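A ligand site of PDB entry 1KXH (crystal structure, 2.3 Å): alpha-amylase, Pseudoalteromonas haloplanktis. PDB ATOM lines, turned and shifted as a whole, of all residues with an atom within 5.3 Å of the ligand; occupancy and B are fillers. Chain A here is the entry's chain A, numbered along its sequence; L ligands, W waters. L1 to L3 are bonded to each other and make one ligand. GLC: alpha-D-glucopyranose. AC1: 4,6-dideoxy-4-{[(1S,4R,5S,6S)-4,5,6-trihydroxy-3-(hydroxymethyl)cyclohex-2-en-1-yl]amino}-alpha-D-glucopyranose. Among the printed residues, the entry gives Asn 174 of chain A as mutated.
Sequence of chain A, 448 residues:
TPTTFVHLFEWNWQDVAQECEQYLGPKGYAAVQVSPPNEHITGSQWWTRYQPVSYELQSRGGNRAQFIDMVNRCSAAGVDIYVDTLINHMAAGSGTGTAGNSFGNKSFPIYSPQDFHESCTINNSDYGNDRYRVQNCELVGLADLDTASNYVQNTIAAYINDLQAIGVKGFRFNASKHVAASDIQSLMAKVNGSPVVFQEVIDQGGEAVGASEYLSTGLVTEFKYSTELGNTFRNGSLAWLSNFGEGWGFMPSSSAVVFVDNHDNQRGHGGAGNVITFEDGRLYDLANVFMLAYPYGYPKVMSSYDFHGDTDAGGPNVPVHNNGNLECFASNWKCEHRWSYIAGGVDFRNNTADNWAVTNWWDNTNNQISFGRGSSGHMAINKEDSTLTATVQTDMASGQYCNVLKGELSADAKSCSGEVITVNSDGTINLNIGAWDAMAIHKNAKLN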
ATOM      1  N   TRP A  46     -10.095  20.346 -15.237  1.00  0.00           N
ATOM      2  CA  TRP A  46     -10.941  19.236 -15.693  1.00  0.00           C
ATOM      3  C   TRP A  46     -10.450  17.899 -15.155  1.00  0.00           C
ATOM      4  O   TRP A  46     -11.253  17.020 -14.884  1.00  0.00           O
ATOM      5  CB  TRP A  46     -11.014  19.148 -17.239  1.00  0.00           C
ATOM      6  CG  TRP A  46      -9.706  18.765 -17.898  1.00  0.00           C
ATOM      7  CD1 TRP A  46      -8.748  19.620 -18.343  1.00  0.00           C
ATOM      8  CD2 TRP A  46      -9.184  17.426 -18.124  1.00  0.00           C
ATOM      9  NE1 TRP A  46      -7.664  18.912 -18.819  1.00  0.00           N
ATOM     10  CE2 TRP A  46      -7.898  17.576 -18.699  1.00  0.00           C
ATOM     11  CE3 TRP A  46      -9.677  16.135 -17.879  1.00  0.00           C
ATOM     12  CZ2 TRP A  46      -7.105  16.474 -19.049  1.00  0.00           C
ATOM     13  CZ3 TRP A  46      -8.878  15.038 -18.234  1.00  0.00           C
ATOM     14  CH2 TRP A  46      -7.606  15.216 -18.817  1.00  0.00           C
ATOM     15  N   TRP A  47      -9.129  17.741 -14.999  1.00  0.00           N
ATOM     16  CA  TRP A  47      -8.560  16.485 -14.511  1.00  0.00           C
ATOM     17  C   TRP A  47      -8.748  16.122 -13.025  1.00  0.00           C
ATOM     18  O   TRP A  47      -8.290  15.072 -12.590  1.00  0.00           O
ATOM     19  CB  TRP A  47      -7.081  16.309 -14.926  1.00  0.00           C
ATOM     20  CG  TRP A  47      -6.149  17.481 -14.656  1.00  0.00           C
ATOM     21  CD1 TRP A  47      -5.569  18.281 -15.605  1.00  0.00           C
ATOM     22  CD2 TRP A  47      -5.646  17.940 -13.391  1.00  0.00           C
ATOM     23  NE1 TRP A  47      -4.747  19.204 -15.012  1.00  0.00           N
ATOM     24  CE2 TRP A  47      -4.765  19.015 -13.649  1.00  0.00           C
ATOM     25  CE3 TRP A  47      -5.846  17.540 -12.049  1.00  0.00           C
ATOM     26  CZ2 TRP A  47      -4.089  19.707 -12.630  1.00  0.00           C
ATOM     27  CZ3 TRP A  47      -5.174  18.227 -11.039  1.00  0.00           C
ATOM     28  CH2 TRP A  47      -4.307  19.299 -11.336  1.00  0.00           C
ATOM     29  N   THR A  48      -9.410  16.988 -12.259  1.00  0.00           N
ATOM     30  CA  THR A  48      -9.632  16.683 -10.847  1.00  0.00           C
ATOM     31  C   THR A  48     -10.585  15.485 -10.761  1.00  0.00           C
ATOM     32  O   THR A  48     -10.539  14.717  -9.810  1.00  0.00           O
ATOM     33  CB  THR A  48     -10.250  17.864 -10.062  1.00  0.00           C
ATOM     34  OG1 THR A  48     -11.536  18.168 -10.603  1.00  0.00           O
ATOM     35  CG2 THR A  48      -9.347  19.084 -10.149  1.00  0.00           C
ATOM     36  N   TYR A  50     -10.396  12.797 -12.201  1.00  0.00           N
ATOM     37  CA  TYR A  50      -9.665  11.546 -12.237  1.00  0.00           C
ATOM     38  C   TYR A  50      -8.842  11.209 -10.982  1.00  0.00           C
ATOM     39  O   TYR A  50      -7.960  10.342 -11.008  1.00  0.00           O
ATOM     40  CB  TYR A  50      -8.832  11.484 -13.528  1.00  0.00           C
ATOM     41  CG  TYR A  50      -9.751  11.437 -14.745  1.00  0.00           C
ATOM     42  CD1 TYR A  50     -10.207  12.610 -15.349  1.00  0.00           C
ATOM     43  CD2 TYR A  50     -10.239  10.219 -15.218  1.00  0.00           C
ATOM     44  CE1 TYR A  50     -11.149  12.571 -16.382  1.00  0.00           C
ATOM     45  CE2 TYR A  50     -11.171  10.165 -16.235  1.00  0.00           C
ATOM     46  CZ  TYR A  50     -11.633  11.335 -16.812  1.00  0.00           C
ATOM     47  OH  TYR A  50     -12.583  11.267 -17.790  1.00  0.00           O
ATOM     48  N   GLN A  51      -9.160  11.904  -9.886  1.00  0.00           N
ATOM     49  CA  GLN A  51      -8.533  11.692  -8.573  1.00  0.00           C
ATOM     50  C   GLN A  51      -9.663  11.509  -7.547  1.00  0.00           C
ATOM     51  O   GLN A  51     -10.138  12.465  -6.929  1.00  0.00           O
ATOM     52  CB  GLN A  51      -7.647  12.886  -8.187  1.00  0.00           C
ATOM     53  CG  GLN A  51      -6.553  13.174  -9.188  1.00  0.00           C
ATOM     54  CD  GLN A  51      -5.447  14.015  -8.617  1.00  0.00           C
ATOM     55  OE1 GLN A  51      -5.055  13.817  -7.460  1.00  0.00           O
ATOM     56  NE2 GLN A  51      -4.913  14.923  -9.420  1.00  0.00           N
ATOM     57  N   LEU A  86     -13.171   4.753 -12.538  1.00  0.00           N
ATOM     58  CA  LEU A  86     -11.766   4.748 -12.147  1.00  0.00           C
ATOM     59  C   LEU A  86     -11.468   3.456 -11.406  1.00  0.00           C
ATOM     60  O   LEU A  86     -11.796   3.320 -10.210  1.00  0.00           O
ATOM     61  CB  LEU A  86     -11.465   5.932 -11.208  1.00  0.00           C
ATOM     62  CG  LEU A  86     -11.419   7.371 -11.727  1.00  0.00           C
ATOM     63  CD1 LEU A  86     -10.266   7.502 -12.665  1.00  0.00           C
ATOM     64  CD2 LEU A  86     -12.705   7.756 -12.426  1.00  0.00           C
ATOM     65  N   HIS A  89      -6.745   3.714  -9.593  1.00  0.00           N
ATOM     66  CA  HIS A  89      -6.125   4.493  -8.534  1.00  0.00           C
ATOM     67  C   HIS A  89      -7.055   5.411  -7.774  1.00  0.00           C
ATOM     68  O   HIS A  89      -8.232   5.549  -8.112  1.00  0.00           O
ATOM     69  CB  HIS A  89      -5.066   5.382  -9.194  1.00  0.00           C
ATOM     70  CG  HIS A  89      -5.597   6.188 -10.350  1.00  0.00           C
ATOM     71  ND1 HIS A  89      -5.551   5.741 -11.653  1.00  0.00           N
ATOM     72  CD2 HIS A  89      -6.263   7.371 -10.380  1.00  0.00           C
ATOM     73  CE1 HIS A  89      -6.160   6.619 -12.440  1.00  0.00           C
ATOM     74  NE2 HIS A  89      -6.604   7.616 -11.688  1.00  0.00           N
ATOM     75  N   ALA A  92      -3.935  11.729  -5.539  1.00  0.00           N
ATOM     76  CA  ALA A  92      -2.550  11.876  -5.093  1.00  0.00           C
ATOM     77  C   ALA A  92      -2.469  12.866  -3.907  1.00  0.00           C
ATOM     78  O   ALA A  92      -3.319  13.759  -3.764  1.00  0.00           O
ATOM     79  CB  ALA A  92      -1.684  12.376  -6.244  1.00  0.00           C
ATOM     80  N   GLY A  93      -1.476  12.663  -3.040  1.00  0.00           N
ATOM     81  CA  GLY A  93      -1.275  13.554  -1.904  1.00  0.00           C
ATOM     82  C   GLY A  93      -2.335  13.564  -0.824  1.00  0.00           C
ATOM     83  O   GLY A  93      -2.721  12.506  -0.310  1.00  0.00           O
ATOM     84  N   LEU A 139       0.903   6.193 -11.713  1.00  0.00           N
ATOM     85  CA  LEU A 139       0.751   7.003 -12.913  1.00  0.00           C
ATOM     86  C   LEU A 139       0.669   8.436 -12.385  1.00  0.00           C
ATOM     87  O   LEU A 139      -0.257   8.782 -11.657  1.00  0.00           O
ATOM     88  CB  LEU A 139      -0.552   6.633 -13.653  1.00  0.00           C
ATOM     89  CG  LEU A 139      -0.956   7.426 -14.892  1.00  0.00           C
ATOM     90  CD1 LEU A 139       0.075   7.293 -15.983  1.00  0.00           C
ATOM     91  CD2 LEU A 139      -2.309   6.923 -15.380  1.00  0.00           C
ATOM     92  N   VAL A 140       1.674   9.249 -12.722  1.00  0.00           N
ATOM     93  CA  VAL A 140       1.763  10.642 -12.272  1.00  0.00           C
ATOM     94  C   VAL A 140       1.412  10.880 -10.783  1.00  0.00           C
ATOM     95  O   VAL A 140       0.655  11.797 -10.430  1.00  0.00           O
ATOM     96  CB  VAL A 140       0.990  11.614 -13.214  1.00  0.00           C
ATOM     97  CG1 VAL A 140       1.590  11.546 -14.606  1.00  0.00           C
ATOM     98  CG2 VAL A 140      -0.496  11.287 -13.277  1.00  0.00           C
ATOM     99  N   GLY A 141       1.933   9.997  -9.920  1.00  0.00           N
ATOM    100  CA  GLY A 141       1.725  10.102  -8.488  1.00  0.00           C
ATOM    101  C   GLY A 141       0.392   9.635  -7.916  1.00  0.00           C
ATOM    102  O   GLY A 141       0.166   9.731  -6.699  1.00  0.00           O
ATOM    103  N   LEU A 142      -0.487   9.113  -8.764  1.00  0.00           N
ATOM    104  CA  LEU A 142      -1.784   8.639  -8.324  1.00  0.00           C
ATOM    105  C   LEU A 142      -1.621   7.337  -7.532  1.00  0.00           C
ATOM    106  O   LEU A 142      -0.944   6.419  -7.982  1.00  0.00           O
ATOM    107  CB  LEU A 142      -2.698   8.434  -9.526  1.00  0.00           C
ATOM    108  CG  LEU A 142      -2.909   9.701 -10.375  1.00  0.00           C
ATOM    109  CD1 LEU A 142      -3.480   9.305 -11.750  1.00  0.00           C
ATOM    110  CD2 LEU A 142      -3.834  10.688  -9.651  1.00  0.00           C
ATOM    111  N   ASN A 174     -11.378   3.442 -17.111  1.00  0.00           N
ATOM    112  CA  ASN A 174     -10.274   4.373 -17.322  1.00  0.00           C
ATOM    113  C   ASN A 174      -8.924   3.773 -16.927  1.00  0.00           C
ATOM    114  O   ASN A 174      -8.841   2.983 -15.993  1.00  0.00           O
ATOM    115  CB  ASN A 174     -10.548   5.643 -16.501  1.00  0.00           C
ATOM    116  CG  ASN A 174      -9.312   6.513 -16.321  1.00  0.00           C
ATOM    117  OD1 ASN A 174      -8.718   6.547 -15.245  1.00  0.00           O
ATOM    118  ND2 ASN A 174      -8.945   7.259 -17.355  1.00  0.00           N
ATOM    119  N   ALA A 175      -7.883   4.116 -17.695  1.00  0.00           N
ATOM    120  CA  ALA A 175      -6.516   3.669 -17.441  1.00  0.00           C
ATOM    121  C   ALA A 175      -6.357   2.150 -17.316  1.00  0.00           C
ATOM    122  O   ALA A 175      -5.580   1.662 -16.493  1.00  0.00           O
ATOM    123  CB  ALA A 175      -5.962   4.380 -16.177  1.00  0.00           C
ATOM    124  N   GLU A 200     -10.353   1.626 -21.717  1.00  0.00           N
ATOM    125  CA  GLU A 200      -9.432   2.584 -22.304  1.00  0.00           C
ATOM    126  C   GLU A 200      -7.999   2.039 -22.293  1.00  0.00           C
ATOM    127  O   GLU A 200      -7.327   2.100 -21.264  1.00  0.00           O
ATOM    128  CB  GLU A 200      -9.469   3.927 -21.572  1.00  0.00           C
ATOM    129  CG  GLU A 200      -8.464   4.953 -22.121  1.00  0.00           C
ATOM    130  CD  GLU A 200      -8.021   5.977 -21.082  1.00  0.00           C
ATOM    131  OE1 GLU A 200      -8.436   5.880 -19.915  1.00  0.00           O
ATOM    132  OE2 GLU A 200      -7.247   6.890 -21.429  1.00  0.00           O
ATOM    133  N   ILE A 202      -4.462   2.419 -24.384  1.00  0.00           N
ATOM    134  CA  ILE A 202      -3.740   3.182 -25.387  1.00  0.00           C
ATOM    135  C   ILE A 202      -2.579   2.325 -25.883  1.00  0.00           C
ATOM    136  O   ILE A 202      -1.608   2.128 -25.165  1.00  0.00           O
ATOM    137  CB  ILE A 202      -3.210   4.528 -24.828  1.00  0.00           C
ATOM    138  CG1 ILE A 202      -4.373   5.326 -24.207  1.00  0.00           C
ATOM    139  CG2 ILE A 202      -2.545   5.338 -25.924  1.00  0.00           C
ATOM    140  CD1 ILE A 202      -3.984   6.703 -23.674  1.00  0.00           C
ATOM    141  N   ASP A 264      -8.778  13.477 -23.964  1.00  0.00           N
ATOM    142  CA  ASP A 264      -7.344  13.463 -23.676  1.00  0.00           C
ATOM    143  C   ASP A 264      -6.505  13.892 -24.876  1.00  0.00           C
ATOM    144  O   ASP A 264      -5.707  14.829 -24.780  1.00  0.00           O
ATOM    145  CB  ASP A 264      -6.862  12.066 -23.248  1.00  0.00           C
ATOM    146  CG  ASP A 264      -7.234  11.719 -21.835  1.00  0.00           C
ATOM    147  OD1 ASP A 264      -6.822  12.444 -20.911  1.00  0.00           O
ATOM    148  OD2 ASP A 264      -7.951  10.721 -21.638  1.00  0.00           O
ATOM    149  N   HIS A 269      -2.649  14.916 -24.401  1.00  0.00           N
ATOM    150  CA  HIS A 269      -2.473  13.709 -23.590  1.00  0.00           C
ATOM    151  C   HIS A 269      -2.683  12.456 -24.415  1.00  0.00           C
ATOM    152  O   HIS A 269      -3.809  12.015 -24.588  1.00  0.00           O
ATOM    153  CB  HIS A 269      -3.453  13.719 -22.413  1.00  0.00           C
ATOM    154  CG  HIS A 269      -3.406  14.947 -21.566  1.00  0.00           C
ATOM    155  ND1 HIS A 269      -2.637  15.040 -20.427  1.00  0.00           N
ATOM    156  CD2 HIS A 269      -4.064  16.131 -21.660  1.00  0.00           C
ATOM    157  CE1 HIS A 269      -2.821  16.219 -19.850  1.00  0.00           C
ATOM    158  NE2 HIS A 269      -3.684  16.896 -20.586  1.00  0.00           N
ATOM    159  N   ASP A 312      -5.200  22.601 -18.990  1.00  0.00           N
ATOM    160  CA  ASP A 312      -5.607  22.159 -17.659  1.00  0.00           C
ATOM    161  C   ASP A 312      -6.989  22.693 -17.269  1.00  0.00           C
ATOM    162  O   ASP A 312      -7.661  22.156 -16.386  1.00  0.00           O
ATOM    163  CB  ASP A 312      -4.617  22.628 -16.582  1.00  0.00           C
ATOM    164  CG  ASP A 312      -3.271  21.975 -16.709  1.00  0.00           C
ATOM    165  OD1 ASP A 312      -2.278  22.722 -16.627  1.00  0.00           O
ATOM    166  OD2 ASP A 312      -3.175  20.739 -16.874  1.00  0.00           O
HETATM  167  C1  GLC L   1      -5.206   7.986 -18.319  1.00  0.00           C
HETATM  168  C2  GLC L   1      -5.211   9.143 -19.310  1.00  0.00           C
HETATM  169  C3  GLC L   1      -4.655  10.376 -18.612  1.00  0.00           C
HETATM  170  C4  GLC L   1      -5.426  10.673 -17.306  1.00  0.00           C
HETATM  171  C5  GLC L   1      -5.551   9.426 -16.430  1.00  0.00           C
HETATM  172  C6  GLC L   1      -6.552   9.685 -15.306  1.00  0.00           C
HETATM  173  O1  GLC L   1      -5.699   6.847 -18.923  1.00  0.00           O
HETATM  174  O2  GLC L   1      -4.395   8.810 -20.414  1.00  0.00           O
HETATM  175  O3  GLC L   1      -4.759  11.494 -19.482  1.00  0.00           O
HETATM  176  O4  GLC L   1      -4.733  11.695 -16.564  1.00  0.00           O
HETATM  177  O5  GLC L   1      -6.047   8.310 -17.199  1.00  0.00           O
HETATM  178  O6  GLC L   1      -6.644   8.591 -14.423  1.00  0.00           O
HETATM  179  C1  GLC L   2      -5.438  12.872 -16.276  1.00  0.00           C
HETATM  180  C2  GLC L   2      -4.633  14.085 -16.783  1.00  0.00           C
HETATM  181  C3  GLC L   2      -3.387  14.306 -15.910  1.00  0.00           C
HETATM  182  C4  GLC L   2      -3.782  14.420 -14.450  1.00  0.00           C
HETATM  183  C5  GLC L   2      -4.543  13.142 -14.049  1.00  0.00           C
HETATM  184  C6  GLC L   2      -4.999  13.089 -12.589  1.00  0.00           C
HETATM  185  O2  GLC L   2      -4.224  13.846 -18.129  1.00  0.00           O
HETATM  186  O3  GLC L   2      -2.719  15.485 -16.317  1.00  0.00           O
HETATM  187  O4  GLC L   2      -2.588  14.588 -13.636  1.00  0.00           O
HETATM  188  O5  GLC L   2      -5.718  13.002 -14.885  1.00  0.00           O
HETATM  189  O6  GLC L   2      -5.739  14.253 -12.244  1.00  0.00           O
HETATM  190  C1  AC1 L   3      -2.632  15.631 -12.695  1.00  0.00           C
HETATM  191  O2  AC1 L   3      -1.539  17.021 -14.293  1.00  0.00           O
HETATM  192  C2  AC1 L   3      -1.502  16.609 -12.940  1.00  0.00           C
HETATM  193  C4A AC1 L   3       4.178  13.892  -8.775  1.00  0.00           C
HETATM  194  C3  AC1 L   3      -0.171  15.930 -12.630  1.00  0.00           C
HETATM  195  O3  AC1 L   3       0.882  16.858 -12.794  1.00  0.00           O
HETATM  196  C4  AC1 L   3      -0.173  15.420 -11.200  1.00  0.00           C
HETATM  197  N4A AC1 L   3       1.106  14.757 -10.935  1.00  0.00           N
HETATM  198  C5  AC1 L   3      -1.362  14.478 -11.007  1.00  0.00           C
HETATM  199  O5  AC1 L   3      -2.584  15.159 -11.353  1.00  0.00           O
HETATM  200  C6  AC1 L   3      -1.448  14.001  -9.570  1.00  0.00           C
HETATM  201  C1B AC1 L   3       1.837  15.549  -9.953  1.00  0.00           C
HETATM  202  C2B AC1 L   3       3.317  15.640 -10.320  1.00  0.00           C
HETATM  203  O2B AC1 L   3       3.434  16.142 -11.640  1.00  0.00           O
HETATM  204  C3B AC1 L   3       3.934  14.252 -10.241  1.00  0.00           C
HETATM  205  O3B AC1 L   3       5.160  14.213 -10.948  1.00  0.00           O
HETATM  206  O4  AC1 L   3       4.654  12.553  -8.683  1.00  0.00           O
HETATM  207  C5B AC1 L   3       2.881  14.103  -8.014  1.00  0.00           C
HETATM  208  C7B AC1 L   3       1.743  14.951  -8.572  1.00  0.00           C
HETATM  209  C6B AC1 L   3       2.694  13.444  -6.658  1.00  0.00           C
HETATM  210  O6B AC1 L   3       2.066  14.352  -5.772  1.00  0.00           O
HETATM  211  O   HOH W   1       1.648  11.252  -4.904  1.00  0.00           O
HETATM  212  O   HOH W   2      -3.847   5.149 -19.924  1.00  0.00           O
HETATM  213  O   HOH W   3      -8.420  11.524 -18.480  1.00  0.00           O
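OD1 of Asp 264 sits at hydrogen-bond distance from O3 of GLC L1, 2.7 Å away. O of Trp 47 is in hydrogen-bond range of O6 of GLC L2 (2.7 Å). NE2 of His 89 lies close to O6 of GLC L1 (2.9 Å). O1 of GLC L1 lies within hydrogen-bond range of OE2 of Glu 200 (2.9 Å). O6 of GLC L2 lies within hydrogen-bond range of NE2 of Gln 51 (3.0 Å). OD1 of Asn 174 sits at hydrogen-bond distance from O6 of GLC L1. A nitrogen (N4A) of AC1 L3 is in hydrogen-bond range of the backbone carbonyl oxygen (O) of Val 140, 3.0 Å away. O2 of GLC L2 sits at hydrogen-bond distance from ND1 of His 269 (3.0 Å).
The backbone NH (N) of His 269 is in hydrogen-bond range of the backbone carbonyl oxygen (O) of Asp 264, 3.1 Å away. The indole nitrogen of Trp 47 sits at hydrogen-bond distance from the side-chain carboxylate of Asp 312, 2.9 Å away. NE2 of His 89 is in hydrogen-bond range of O of Tyr 50 (3.1 Å). The side-chain carboxylate of Glu 200 sits at hydrogen-bond distance from the side-chain amide nitrogen of Asn 174 (3.0 Å). N of Ala 175 is in hydrogen-bond range of OE1 of Glu 200 (2.9 Å). The backbone NH (N) of Ala 92 sits at hydrogen-bond distance from the side-chain amide oxygen (OE1) of Gln 51 (3.1 Å). The backbone NH of Trp 46 sits at hydrogen-bond distance from the backbone carbonyl oxygen of Asp 312, at 3.2 Å.
CH2 of Trp 46 touches O2 of GLC L2, 3.7 Å away. CB of Tyr 50 touches C6 of GLC L1, 3.4 Å away. Ala 92 touches the ligand. CA of Gly 141 touches O4 of AC1 L3, at 3.8 Å. CD2 of Leu 142 touches C6 of GLC L2, at 3.97 Å. Ala 175 touches the ligand. CD1 of Ile 202 touches O2 of GLC L1, at 3.9 Å. Hydrophobic or aromatic side chains within 4 Å of the ligand: Trp 46, Trp 47, Tyr 50, His 89, Ala 92, Val 140, Leu 142, Ala 175, Ile 202 and His 269. 15 residues have an atom within 4 Å of the ligand: Trp 46, Trp 47, Tyr 50, Gln 51, His 89, Ala 92, Val 140, Gly 141, Leu 142, Asn 174, Ala 175, Glu 200, Ile 202, Asp 264 and His 269. The nearest printed residue that does not touch the ligand is Leu 86 (4.2 Å).
Water W1 bridges O of Gly 141 (2.8 Å) and O6B of AC1 L3 (3.2 Å).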
